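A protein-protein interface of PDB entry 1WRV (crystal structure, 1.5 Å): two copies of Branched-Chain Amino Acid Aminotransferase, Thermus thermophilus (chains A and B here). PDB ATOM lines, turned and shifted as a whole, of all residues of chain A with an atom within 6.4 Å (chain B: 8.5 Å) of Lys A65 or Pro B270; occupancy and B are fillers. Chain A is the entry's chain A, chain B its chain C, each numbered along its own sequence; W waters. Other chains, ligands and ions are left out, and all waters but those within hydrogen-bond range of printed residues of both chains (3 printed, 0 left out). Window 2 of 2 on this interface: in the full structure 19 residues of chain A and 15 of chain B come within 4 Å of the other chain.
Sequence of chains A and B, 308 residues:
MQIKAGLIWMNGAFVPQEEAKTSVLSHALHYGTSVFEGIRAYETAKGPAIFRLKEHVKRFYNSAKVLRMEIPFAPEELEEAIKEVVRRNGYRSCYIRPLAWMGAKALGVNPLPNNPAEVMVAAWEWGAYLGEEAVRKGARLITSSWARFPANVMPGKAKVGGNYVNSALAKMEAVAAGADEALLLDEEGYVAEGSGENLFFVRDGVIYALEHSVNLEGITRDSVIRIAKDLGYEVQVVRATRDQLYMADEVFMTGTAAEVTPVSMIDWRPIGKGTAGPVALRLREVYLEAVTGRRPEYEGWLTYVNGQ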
ATOM      1  N   VAL A  35      15.134 -20.445 -17.403  1.00  0.00           N
ATOM      2  CA  VAL A  35      16.379 -20.800 -16.733  1.00  0.00           C
ATOM      3  C   VAL A  35      16.117 -22.139 -16.062  1.00  0.00           C
ATOM      4  O   VAL A  35      15.004 -22.412 -15.618  1.00  0.00           O
ATOM      5  CB  VAL A  35      16.817 -19.759 -15.670  1.00  0.00           C
ATOM      6  CG1 VAL A  35      17.148 -18.443 -16.345  1.00  0.00           C
ATOM      7  CG2 VAL A  35      15.728 -19.567 -14.628  1.00  0.00           C
ATOM      8  N   PHE A  60      20.541 -21.044  -9.813  1.00  0.00           N
ATOM      9  CA  PHE A  60      19.221 -20.950 -10.426  1.00  0.00           C
ATOM     10  C   PHE A  60      18.776 -19.492 -10.342  1.00  0.00           C
ATOM     11  O   PHE A  60      18.328 -18.904 -11.331  1.00  0.00           O
ATOM     12  CB  PHE A  60      18.232 -21.845  -9.669  1.00  0.00           C
ATOM     13  CG  PHE A  60      16.875 -21.963 -10.323  1.00  0.00           C
ATOM     14  CD1 PHE A  60      16.704 -22.680 -11.505  1.00  0.00           C
ATOM     15  CD2 PHE A  60      15.754 -21.384  -9.731  1.00  0.00           C
ATOM     16  CE1 PHE A  60      15.431 -22.818 -12.085  1.00  0.00           C
ATOM     17  CE2 PHE A  60      14.485 -21.517 -10.300  1.00  0.00           C
ATOM     18  CZ  PHE A  60      14.323 -22.235 -11.478  1.00  0.00           C
ATOM     19  N   TYR A  61      18.914 -18.903  -9.158  1.00  0.00           N
ATOM     20  CA  TYR A  61      18.528 -17.512  -8.963  1.00  0.00           C
ATOM     21  C   TYR A  61      19.484 -16.559  -9.671  1.00  0.00           C
ATOM     22  O   TYR A  61      19.071 -15.500 -10.143  1.00  0.00           O
ATOM     23  CB  TYR A  61      18.436 -17.172  -7.470  1.00  0.00           C
ATOM     24  CG  TYR A  61      17.160 -17.675  -6.831  1.00  0.00           C
ATOM     25  CD1 TYR A  61      16.994 -19.023  -6.528  1.00  0.00           C
ATOM     26  CD2 TYR A  61      16.095 -16.807  -6.580  1.00  0.00           C
ATOM     27  CE1 TYR A  61      15.801 -19.499  -5.993  1.00  0.00           C
ATOM     28  CE2 TYR A  61      14.896 -17.273  -6.048  1.00  0.00           C
ATOM     29  CZ  TYR A  61      14.757 -18.620  -5.758  1.00  0.00           C
ATOM     30  OH  TYR A  61      13.579 -19.095  -5.227  1.00  0.00           O
ATOM     31  N   ASN A  62      20.756 -16.937  -9.749  1.00  0.00           N
ATOM     32  CA  ASN A  62      21.737 -16.102 -10.440  1.00  0.00           C
ATOM     33  C   ASN A  62      21.411 -16.080 -11.931  1.00  0.00           C
ATOM     34  O   ASN A  62      21.526 -15.044 -12.581  1.00  0.00           O
ATOM     35  CB  ASN A  62      23.156 -16.636 -10.201  1.00  0.00           C
ATOM     36  CG  ASN A  62      23.748 -16.148  -8.891  1.00  0.00           C
ATOM     37  OD1 ASN A  62      24.720 -16.712  -8.379  1.00  0.00           O
ATOM     38  ND2 ASN A  62      23.173 -15.082  -8.349  1.00  0.00           N
ATOM     39  N   SER A  63      20.994 -17.221 -12.474  1.00  0.00           N
ATOM     40  CA  SER A  63      20.637 -17.284 -13.887  1.00  0.00           C
ATOM     41  C   SER A  63      19.441 -16.378 -14.156  1.00  0.00           C
ATOM     42  O   SER A  63      19.404 -15.661 -15.156  1.00  0.00           O
ATOM     43  CB  SER A  63      20.309 -18.724 -14.298  1.00  0.00           C
ATOM     44  OG  SER A  63      21.480 -19.528 -14.299  1.00  0.00           O
ATOM     45  N   ALA A  64      18.463 -16.401 -13.257  1.00  0.00           N
ATOM     46  CA  ALA A  64      17.284 -15.558 -13.422  1.00  0.00           C
ATOM     47  C   ALA A  64      17.674 -14.081 -13.428  1.00  0.00           C
ATOM     48  O   ALA A  64      17.145 -13.297 -14.222  1.00  0.00           O
ATOM     49  CB  ALA A  64      16.286 -15.829 -12.303  1.00  0.00           C
ATOM     50  N   LYS A  65      18.605 -13.708 -12.553  1.00  0.00           N
ATOM     51  CA  LYS A  65      19.042 -12.317 -12.478  1.00  0.00           C
ATOM     52  C   LYS A  65      19.628 -11.842 -13.797  1.00  0.00           C
ATOM     53  O   LYS A  65      19.454 -10.686 -14.171  1.00  0.00           O
ATOM     54  CB  LYS A  65      20.083 -12.110 -11.380  1.00  0.00           C
ATOM     55  CG  LYS A  65      20.570 -10.661 -11.327  1.00  0.00           C
ATOM     56  CD  LYS A  65      21.718 -10.470 -10.363  1.00  0.00           C
ATOM     57  CE  LYS A  65      21.303 -10.725  -8.931  1.00  0.00           C
ATOM     58  NZ  LYS A  65      22.467 -10.579  -8.015  1.00  0.00           N
ATOM     59  N   VAL A  66      20.336 -12.724 -14.496  1.00  0.00           N
ATOM     60  CA  VAL A  66      20.915 -12.351 -15.779  1.00  0.00           C
ATOM     61  C   VAL A  66      19.815 -11.913 -16.742  1.00  0.00           C
ATOM     62  O   VAL A  66      20.000 -10.983 -17.524  1.00  0.00           O
ATOM     63  CB  VAL A  66      21.698 -13.525 -16.415  1.00  0.00           C
ATOM     64  CG1 VAL A  66      22.274 -13.102 -17.751  1.00  0.00           C
ATOM     65  CG2 VAL A  66      22.813 -13.958 -15.500  1.00  0.00           C
ATOM     66  N   LEU A  67      18.666 -12.582 -16.685  1.00  0.00           N
ATOM     67  CA  LEU A  67      17.546 -12.247 -17.560  1.00  0.00           C
ATOM     68  C   LEU A  67      16.623 -11.219 -16.930  1.00  0.00           C
ATOM     69  O   LEU A  67      15.603 -10.867 -17.514  1.00  0.00           O
ATOM     70  CB  LEU A  67      16.708 -13.488 -17.866  1.00  0.00           C
ATOM     71  CG  LEU A  67      17.302 -14.580 -18.753  1.00  0.00           C
ATOM     72  CD1 LEU A  67      16.291 -15.708 -18.879  1.00  0.00           C
ATOM     73  CD2 LEU A  67      17.640 -14.016 -20.124  1.00  0.00           C
ATOM     74  N   ARG A  68      16.982 -10.748 -15.740  1.00  0.00           N
ATOM     75  CA  ARG A  68      16.150  -9.799 -15.011  1.00  0.00           C
ATOM     76  C   ARG A  68      14.789 -10.451 -14.786  1.00  0.00           C
ATOM     77  O   ARG A  68      13.749  -9.794 -14.762  1.00  0.00           O
ATOM     78  CB  ARG A  68      16.030  -8.480 -15.778  1.00  0.00           C
ATOM     79  CG  ARG A  68      17.345  -7.704 -15.792  1.00  0.00           C
ATOM     80  CD  ARG A  68      17.173  -6.314 -16.381  1.00  0.00           C
ATOM     81  NE  ARG A  68      16.310  -5.475 -15.559  1.00  0.00           N
ATOM     82  CZ  ARG A  68      15.858  -4.285 -15.935  1.00  0.00           C
ATOM     83  NH1 ARG A  68      16.192  -3.800 -17.124  1.00  0.00           N
ATOM     84  NH2 ARG A  68      15.073  -3.583 -15.130  1.00  0.00           N
ATOM     85  N   MET A  69      14.830 -11.770 -14.618  1.00  0.00           N
ATOM     86  CA  MET A  69      13.651 -12.589 -14.378  1.00  0.00           C
ATOM     87  C   MET A  69      13.407 -12.648 -12.877  1.00  0.00           C
ATOM     88  O   MET A  69      14.344 -12.834 -12.093  1.00  0.00           O
ATOM     89  CB  MET A  69      13.893 -14.003 -14.917  1.00  0.00           C
ATOM     90  CG  MET A  69      12.856 -15.016 -14.492  1.00  0.00           C
ATOM     91  SD  MET A  69      13.334 -16.695 -14.920  1.00  0.00           S
ATOM     92  CE  MET A  69      12.856 -16.755 -16.633  1.00  0.00           C
ATOM     93  N   ASP B 243      28.508 -11.569 -16.804  1.00  0.00           N
ATOM     94  CA  ASP B 243      27.653 -12.300 -15.888  1.00  0.00           C
ATOM     95  C   ASP B 243      28.389 -12.886 -14.690  1.00  0.00           C
ATOM     96  O   ASP B 243      27.760 -13.289 -13.718  1.00  0.00           O
ATOM     97  CB  ASP B 243      26.771 -13.350 -16.606  1.00  0.00           C
ATOM     98  CG  ASP B 243      27.479 -14.124 -17.709  1.00  0.00           C
ATOM     99  OD1 ASP B 243      28.587 -13.753 -18.154  1.00  0.00           O
ATOM    100  OD2 ASP B 243      26.873 -15.126 -18.150  1.00  0.00           O
ATOM    101  N   LEU B 245      30.317 -11.011 -13.069  1.00  0.00           N
ATOM    102  CA  LEU B 245      30.183  -9.851 -12.197  1.00  0.00           C
ATOM    103  C   LEU B 245      28.757  -9.784 -11.646  1.00  0.00           C
ATOM    104  O   LEU B 245      28.566  -9.541 -10.459  1.00  0.00           O
ATOM    105  CB  LEU B 245      30.506  -8.556 -12.950  1.00  0.00           C
ATOM    106  CG  LEU B 245      31.904  -8.411 -13.562  1.00  0.00           C
ATOM    107  CD1 LEU B 245      32.115  -6.961 -13.997  1.00  0.00           C
ATOM    108  CD2 LEU B 245      32.960  -8.814 -12.558  1.00  0.00           C
ATOM    109  N   TYR B 246      27.764 -10.010 -12.508  1.00  0.00           N
ATOM    110  CA  TYR B 246      26.358  -9.978 -12.086  1.00  0.00           C
ATOM    111  C   TYR B 246      26.110 -10.893 -10.896  1.00  0.00           C
ATOM    112  O   TYR B 246      25.305 -10.574 -10.028  1.00  0.00           O
ATOM    113  CB  TYR B 246      25.425 -10.456 -13.200  1.00  0.00           C
ATOM    114  CG  TYR B 246      25.353  -9.616 -14.455  1.00  0.00           C
ATOM    115  CD1 TYR B 246      24.885 -10.180 -15.636  1.00  0.00           C
ATOM    116  CD2 TYR B 246      25.739  -8.273 -14.471  1.00  0.00           C
ATOM    117  CE1 TYR B 246      24.805  -9.449 -16.804  1.00  0.00           C
ATOM    118  CE2 TYR B 246      25.660  -7.522 -15.646  1.00  0.00           C
ATOM    119  CZ  TYR B 246      25.190  -8.125 -16.811  1.00  0.00           C
ATOM    120  OH  TYR B 246      25.100  -7.430 -17.991  1.00  0.00           O
ATOM    121  N   MET B 247      26.793 -12.036 -10.879  1.00  0.00           N
ATOM    122  CA  MET B 247      26.630 -13.033  -9.821  1.00  0.00           C
ATOM    123  C   MET B 247      27.618 -12.916  -8.661  1.00  0.00           C
ATOM    124  O   MET B 247      27.586 -13.724  -7.732  1.00  0.00           O
ATOM    125  CB  MET B 247      26.746 -14.446 -10.407  1.00  0.00           C
ATOM    126  CG  MET B 247      25.722 -14.808 -11.475  1.00  0.00           C
ATOM    127  SD  MET B 247      26.057 -16.437 -12.200  1.00  0.00           S
ATOM    128  CE  MET B 247      26.354 -15.974 -13.847  1.00  0.00           C
ATOM    129  N   ALA B 248      28.500 -11.929  -8.711  1.00  0.00           N
ATOM    130  CA  ALA B 248      29.487 -11.755  -7.651  1.00  0.00           C
ATOM    131  C   ALA B 248      28.842 -11.256  -6.366  1.00  0.00           C
ATOM    132  O   ALA B 248      27.758 -10.674  -6.395  1.00  0.00           O
ATOM    133  CB  ALA B 248      30.565 -10.771  -8.107  1.00  0.00           C
ATOM    134  N   ASP B 249      29.504 -11.489  -5.236  1.00  0.00           N
ATOM    135  CA  ASP B 249      28.983 -11.014  -3.959  1.00  0.00           C
ATOM    136  C   ASP B 249      29.227  -9.513  -3.888  1.00  0.00           C
ATOM    137  O   ASP B 249      28.450  -8.772  -3.284  1.00  0.00           O
ATOM    138  CB  ASP B 249      29.682 -11.705  -2.785  1.00  0.00           C
ATOM    139  CG  ASP B 249      29.346 -13.186  -2.690  1.00  0.00           C
ATOM    140  OD1 ASP B 249      28.221 -13.570  -3.068  1.00  0.00           O
ATOM    141  OD2 ASP B 249      30.201 -13.961  -2.221  1.00  0.00           O
ATOM    142  N   GLU B 250      30.316  -9.080  -4.516  1.00  0.00           N
ATOM    143  CA  GLU B 250      30.689  -7.674  -4.567  1.00  0.00           C
ATOM    144  C   GLU B 250      31.478  -7.385  -5.833  1.00  0.00           C
ATOM    145  O   GLU B 250      32.083  -8.277  -6.429  1.00  0.00           O
ATOM    146  CB  GLU B 250      31.576  -7.285  -3.380  1.00  0.00           C
ATOM    147  CG  GLU B 250      30.899  -7.231  -2.030  1.00  0.00           C
ATOM    148  CD  GLU B 250      31.829  -6.685  -0.953  1.00  0.00           C
ATOM    149  OE1 GLU B 250      32.446  -5.621  -1.181  1.00  0.00           O
ATOM    150  OE2 GLU B 250      31.938  -7.311   0.119  1.00  0.00           O
ATOM    151  N   VAL B 251      31.459  -6.123  -6.234  1.00  0.00           N
ATOM    152  CA  VAL B 251      32.220  -5.647  -7.380  1.00  0.00           C
ATOM    153  C   VAL B 251      32.712  -4.266  -6.969  1.00  0.00           C
ATOM    154  O   VAL B 251      31.997  -3.527  -6.297  1.00  0.00           O
ATOM    155  CB  VAL B 251      31.344  -5.495  -8.652  1.00  0.00           C
ATOM    156  CG1 VAL B 251      32.145  -4.816  -9.764  1.00  0.00           C
ATOM    157  CG2 VAL B 251      30.855  -6.862  -9.121  1.00  0.00           C
ATOM    158  N   VAL B 263      30.829  -1.051  -6.286  1.00  0.00           N
ATOM    159  CA  VAL B 263      29.843  -1.043  -7.365  1.00  0.00           C
ATOM    160  C   VAL B 263      28.636  -1.839  -6.874  1.00  0.00           C
ATOM    161  O   VAL B 263      28.725  -3.048  -6.647  1.00  0.00           O
ATOM    162  CB  VAL B 263      30.414  -1.694  -8.648  1.00  0.00           C
ATOM    163  CG1 VAL B 263      29.310  -1.861  -9.688  1.00  0.00           C
ATOM    164  CG2 VAL B 263      31.538  -0.830  -9.209  1.00  0.00           C
ATOM    165  N   SER B 264      27.511  -1.154  -6.706  1.00  0.00           N
ATOM    166  CA  SER B 264      26.297  -1.792  -6.207  1.00  0.00           C
ATOM    167  C   SER B 264      25.353  -2.333  -7.277  1.00  0.00           C
ATOM    168  O   SER B 264      24.471  -3.138  -6.974  1.00  0.00           O
ATOM    169  CB  SER B 264      25.536  -0.815  -5.309  1.00  0.00           C
ATOM    170  OG  SER B 264      25.114   0.316  -6.041  1.00  0.00           O
ATOM    171  N   MET B 265      25.530  -1.896  -8.519  1.00  0.00           N
ATOM    172  CA  MET B 265      24.657  -2.341  -9.598  1.00  0.00           C
ATOM    173  C   MET B 265      25.329  -2.248 -10.961  1.00  0.00           C
ATOM    174  O   MET B 265      26.068  -1.298 -11.234  1.00  0.00           O
ATOM    175  CB  MET B 265      23.385  -1.487  -9.586  1.00  0.00           C
ATOM    176  CG  MET B 265      22.393  -1.773 -10.699  1.00  0.00           C
ATOM    177  SD  MET B 265      20.860  -0.836 -10.440  1.00  0.00           S
ATOM    178  CE  MET B 265      20.156  -1.801  -9.163  1.00  0.00           C
ATOM    179  N   ILE B 266      25.073  -3.241 -11.809  1.00  0.00           N
ATOM    180  CA  ILE B 266      25.614  -3.259 -13.164  1.00  0.00           C
ATOM    181  C   ILE B 266      24.475  -3.645 -14.100  1.00  0.00           C
ATOM    182  O   ILE B 266      23.833  -4.680 -13.910  1.00  0.00           O
ATOM    183  CB  ILE B 266      26.755  -4.294 -13.345  1.00  0.00           C
ATOM    184  CG1 ILE B 266      27.893  -4.018 -12.352  1.00  0.00           C
ATOM    185  CG2 ILE B 266      27.275  -4.224 -14.776  1.00  0.00           C
ATOM    186  CD1 ILE B 266      29.047  -5.010 -12.432  1.00  0.00           C
ATOM    187  N   ASP B 267      24.223  -2.811 -15.103  1.00  0.00           N
ATOM    188  CA  ASP B 267      23.159  -3.064 -16.066  1.00  0.00           C
ATOM    189  C   ASP B 267      21.812  -3.282 -15.375  1.00  0.00           C
ATOM    190  O   ASP B 267      21.046  -4.186 -15.716  1.00  0.00           O
ATOM    191  CB  ASP B 267      23.520  -4.266 -16.952  1.00  0.00           C
ATOM    192  CG  ASP B 267      24.759  -4.010 -17.800  1.00  0.00           C
ATOM    193  OD1 ASP B 267      24.996  -2.843 -18.167  1.00  0.00           O
ATOM    194  OD2 ASP B 267      25.490  -4.972 -18.115  1.00  0.00           O
ATOM    195  N   TRP B 268      21.539  -2.434 -14.391  1.00  0.00           N
ATOM    196  CA  TRP B 268      20.288  -2.477 -13.641  1.00  0.00           C
ATOM    197  C   TRP B 268      20.079  -3.781 -12.886  1.00  0.00           C
ATOM    198  O   TRP B 268      18.973  -4.084 -12.442  1.00  0.00           O
ATOM    199  CB  TRP B 268      19.121  -2.204 -14.588  1.00  0.00           C
ATOM    200  CG  TRP B 268      19.402  -1.025 -15.472  1.00  0.00           C
ATOM    201  CD1 TRP B 268      19.487  -1.028 -16.832  1.00  0.00           C
ATOM    202  CD2 TRP B 268      19.731   0.303 -15.052  1.00  0.00           C
ATOM    203  NE1 TRP B 268      19.859   0.213 -17.288  1.00  0.00           N
ATOM    204  CE2 TRP B 268      20.016   1.051 -16.217  1.00  0.00           C
ATOM    205  CE3 TRP B 268      19.822   0.933 -13.804  1.00  0.00           C
ATOM    206  CZ2 TRP B 268      20.385   2.401 -16.171  1.00  0.00           C
ATOM    207  CZ3 TRP B 268      20.194   2.278 -13.755  1.00  0.00           C
ATOM    208  CH2 TRP B 268      20.471   2.996 -14.934  1.00  0.00           C
ATOM    209  N   ARG B 269      21.148  -4.555 -12.745  1.00  0.00           N
ATOM    210  CA  ARG B 269      21.086  -5.812 -12.011  1.00  0.00           C
ATOM    211  C   ARG B 269      21.883  -5.581 -10.726  1.00  0.00           C
ATOM    212  O   ARG B 269      23.076  -5.287 -10.770  1.00  0.00           O
ATOM    213  CB  ARG B 269      21.696  -6.938 -12.848  1.00  0.00           C
ATOM    214  CG  ARG B 269      20.930  -7.206 -14.140  1.00  0.00           C
ATOM    215  CD  ARG B 269      21.738  -8.091 -15.072  1.00  0.00           C
ATOM    216  NE  ARG B 269      20.978  -8.567 -16.226  1.00  0.00           N
ATOM    217  CZ  ARG B 269      20.580  -7.814 -17.250  1.00  0.00           C
ATOM    218  NH1 ARG B 269      20.849  -6.516 -17.291  1.00  0.00           N
ATOM    219  NH2 ARG B 269      19.932  -8.375 -18.260  1.00  0.00           N
ATOM    220  N   PRO B 270      21.225  -5.695  -9.560  1.00  0.00           N
ATOM    221  CA  PRO B 270      21.922  -5.481  -8.288  1.00  0.00           C
ATOM    222  C   PRO B 270      23.038  -6.483  -8.050  1.00  0.00           C
ATOM    223  O   PRO B 270      22.912  -7.666  -8.372  1.00  0.00           O
ATOM    224  CB  PRO B 270      20.801  -5.607  -7.258  1.00  0.00           C
ATOM    225  CG  PRO B 270      19.898  -6.618  -7.885  1.00  0.00           C
ATOM    226  CD  PRO B 270      19.847  -6.167  -9.331  1.00  0.00           C
ATOM    227  N   ILE B 271      24.136  -5.997  -7.483  1.00  0.00           N
ATOM    228  CA  ILE B 271      25.269  -6.852  -7.180  1.00  0.00           C
ATOM    229  C   ILE B 271      25.144  -7.266  -5.721  1.00  0.00           C
ATOM    230  O   ILE B 271      25.202  -6.425  -4.819  1.00  0.00           O
ATOM    231  CB  ILE B 271      26.607  -6.110  -7.395  1.00  0.00           C
ATOM    232  CG1 ILE B 271      26.710  -5.641  -8.851  1.00  0.00           C
ATOM    233  CG2 ILE B 271      27.773  -7.021  -7.038  1.00  0.00           C
ATOM    234  CD1 ILE B 271      26.502  -6.749  -9.889  1.00  0.00           C
ATOM    235  N   GLY B 272      24.953  -8.560  -5.496  1.00  0.00           N
ATOM    236  CA  GLY B 272      24.816  -9.055  -4.141  1.00  0.00           C
ATOM    237  C   GLY B 272      23.663  -8.388  -3.419  1.00  0.00           C
ATOM    238  O   GLY B 272      22.517  -8.489  -3.844  1.00  0.00           O
ATOM    239  N   LYS B 273      23.986  -7.688  -2.336  1.00  0.00           N
ATOM    240  CA  LYS B 273      23.004  -6.990  -1.510  1.00  0.00           C
ATOM    241  C   LYS B 273      22.388  -5.780  -2.216  1.00  0.00           C
ATOM    242  O   LYS B 273      21.381  -5.237  -1.765  1.00  0.00           O
ATOM    243  CB  LYS B 273      23.673  -6.508  -0.216  1.00  0.00           C
ATOM    244  CG  LYS B 273      24.887  -7.330   0.227  1.00  0.00           C
ATOM    245  CD  LYS B 273      26.007  -6.440   0.796  1.00  0.00           C
ATOM    246  CE  LYS B 273      26.133  -6.537   2.311  1.00  0.00           C
ATOM    247  NZ  LYS B 273      26.814  -7.799   2.748  1.00  0.00           N
ATOM    248  N   GLY B 274      22.997  -5.338  -3.313  1.00  0.00           N
ATOM    249  CA  GLY B 274      22.458  -4.188  -4.018  1.00  0.00           C
ATOM    250  C   GLY B 274      22.980  -2.875  -3.458  1.00  0.00           C
ATOM    251  O   GLY B 274      22.546  -1.791  -3.863  1.00  0.00           O
ATOM    252  N   THR B 275      23.916  -2.975  -2.519  1.00  0.00           N
ATOM    253  CA  THR B 275      24.537  -1.808  -1.896  1.00  0.00           C
ATOM    254  C   THR B 275      26.014  -2.116  -1.710  1.00  0.00           C
ATOM    255  O   THR B 275      26.444  -3.242  -1.947  1.00  0.00           O
ATOM    256  CB  THR B 275      23.947  -1.513  -0.505  1.00  0.00           C
ATOM    257  OG1 THR B 275      24.380  -2.521   0.419  1.00  0.00           O
ATOM    258  CG2 THR B 275      22.429  -1.496  -0.566  1.00  0.00           C
HETATM  259  O   HOH W   1      25.936 -15.264  -6.238  1.00  0.00           O
HETATM  260  O   HOH W   2      17.093  -6.157 -12.362  1.00  0.00           O
HETATM  261  O   HOH W   3      25.264 -10.596  -7.349  1.00  0.00           O
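No residue of chain B comes within 4 Å of Ala A64.
Printed residues of chain B within 4 Å of Lys A65: Tyr B246 (3.5 Å), Arg B269 (3.3 Å) and Pro B270 (3.0 Å).
Of the printed residues of chain B, Val A66 touches Arg B269.
Of the printed residues of chain A, Tyr B246 touches Lys A65 (3.5 Å).
Of the printed residues of chain A, Arg B269 touches Lys A65 (3.3 Å), Val A66 (2.7 Å) and Arg A68 (3.6 Å).
The nearest printed residue of chain A that does not touch Met B247 is Val A66 (4.4 Å).
OH of Tyr B246 lies within hydrogen-bond range of OD2 of Asp B267 (2.5 Å).
NH1 of Arg B269 is in hydrogen-bond range of O of Asp B267.
No position is printed for both chains.
Of the 6 pairs that touch across the chains among the printed residues, none has its exchanged pair printed and touching as well.
Water W3 lies within hydrogen-bond range of the backbone carbonyl oxygen (O) of Ala B248 (2.7 Å), the backbone carbonyl oxygen (O) of Tyr B246 (2.7 Å), the backbone NH (N) of Gly B272 (2.8 Å) and the side-chain amino group (NZ) of Lys A65 (2.9 Å).
Water W1 bridges O of Met B247 (2.7 Å) and OD1 of Asn A62 (2.9 Å).
Water W2 lies within hydrogen-bond range of the backbone carbonyl oxygen (O) of Trp B268 and the guanidinium group (NE) of Arg A68.
Of the 11 printed residues of chain A, 4 touch a printed residue of chain B.
Of the 21 printed residues of chain B, 4 touch a printed residue of chain A.
Printed residues of chain B that touch a printed residue of chain A: Tyr B246, Met B247, Arg B269 and Pro B270.
Hydrophobic or aromatic side chains of chain B that line the printed part of chain A: Met B247.
Among the printed residues, 6 pairs touch across the chains.
Among the printed residues, no Asp or Glu carboxylate lies within 4 Å of a Lys or Arg side-chain nitrogen of the other chain.
The backbone carbonyl oxygen (O) of Tyr B246 sits at hydrogen-bond distance from the side-chain amino group (NZ) of Lys A65, 3.5 Å away.
The guanidinium group (NE) of Arg B269 sits at hydrogen-bond distance from the backbone carbonyl oxygen (O) of Lys A65.
NZ of Lys A65 is in hydrogen-bond range of O of Pro B270 (3.0 Å).
The backbone carbonyl oxygen of Val A66 sits at hydrogen-bond distance from the guanidinium group of Arg B269 (2.7 Å).
Asn A62 touches Met B247 (CB to CG, 3.4 Å).
Arg A68 touches Arg B269 (CG to CZ, 3.6 Å).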
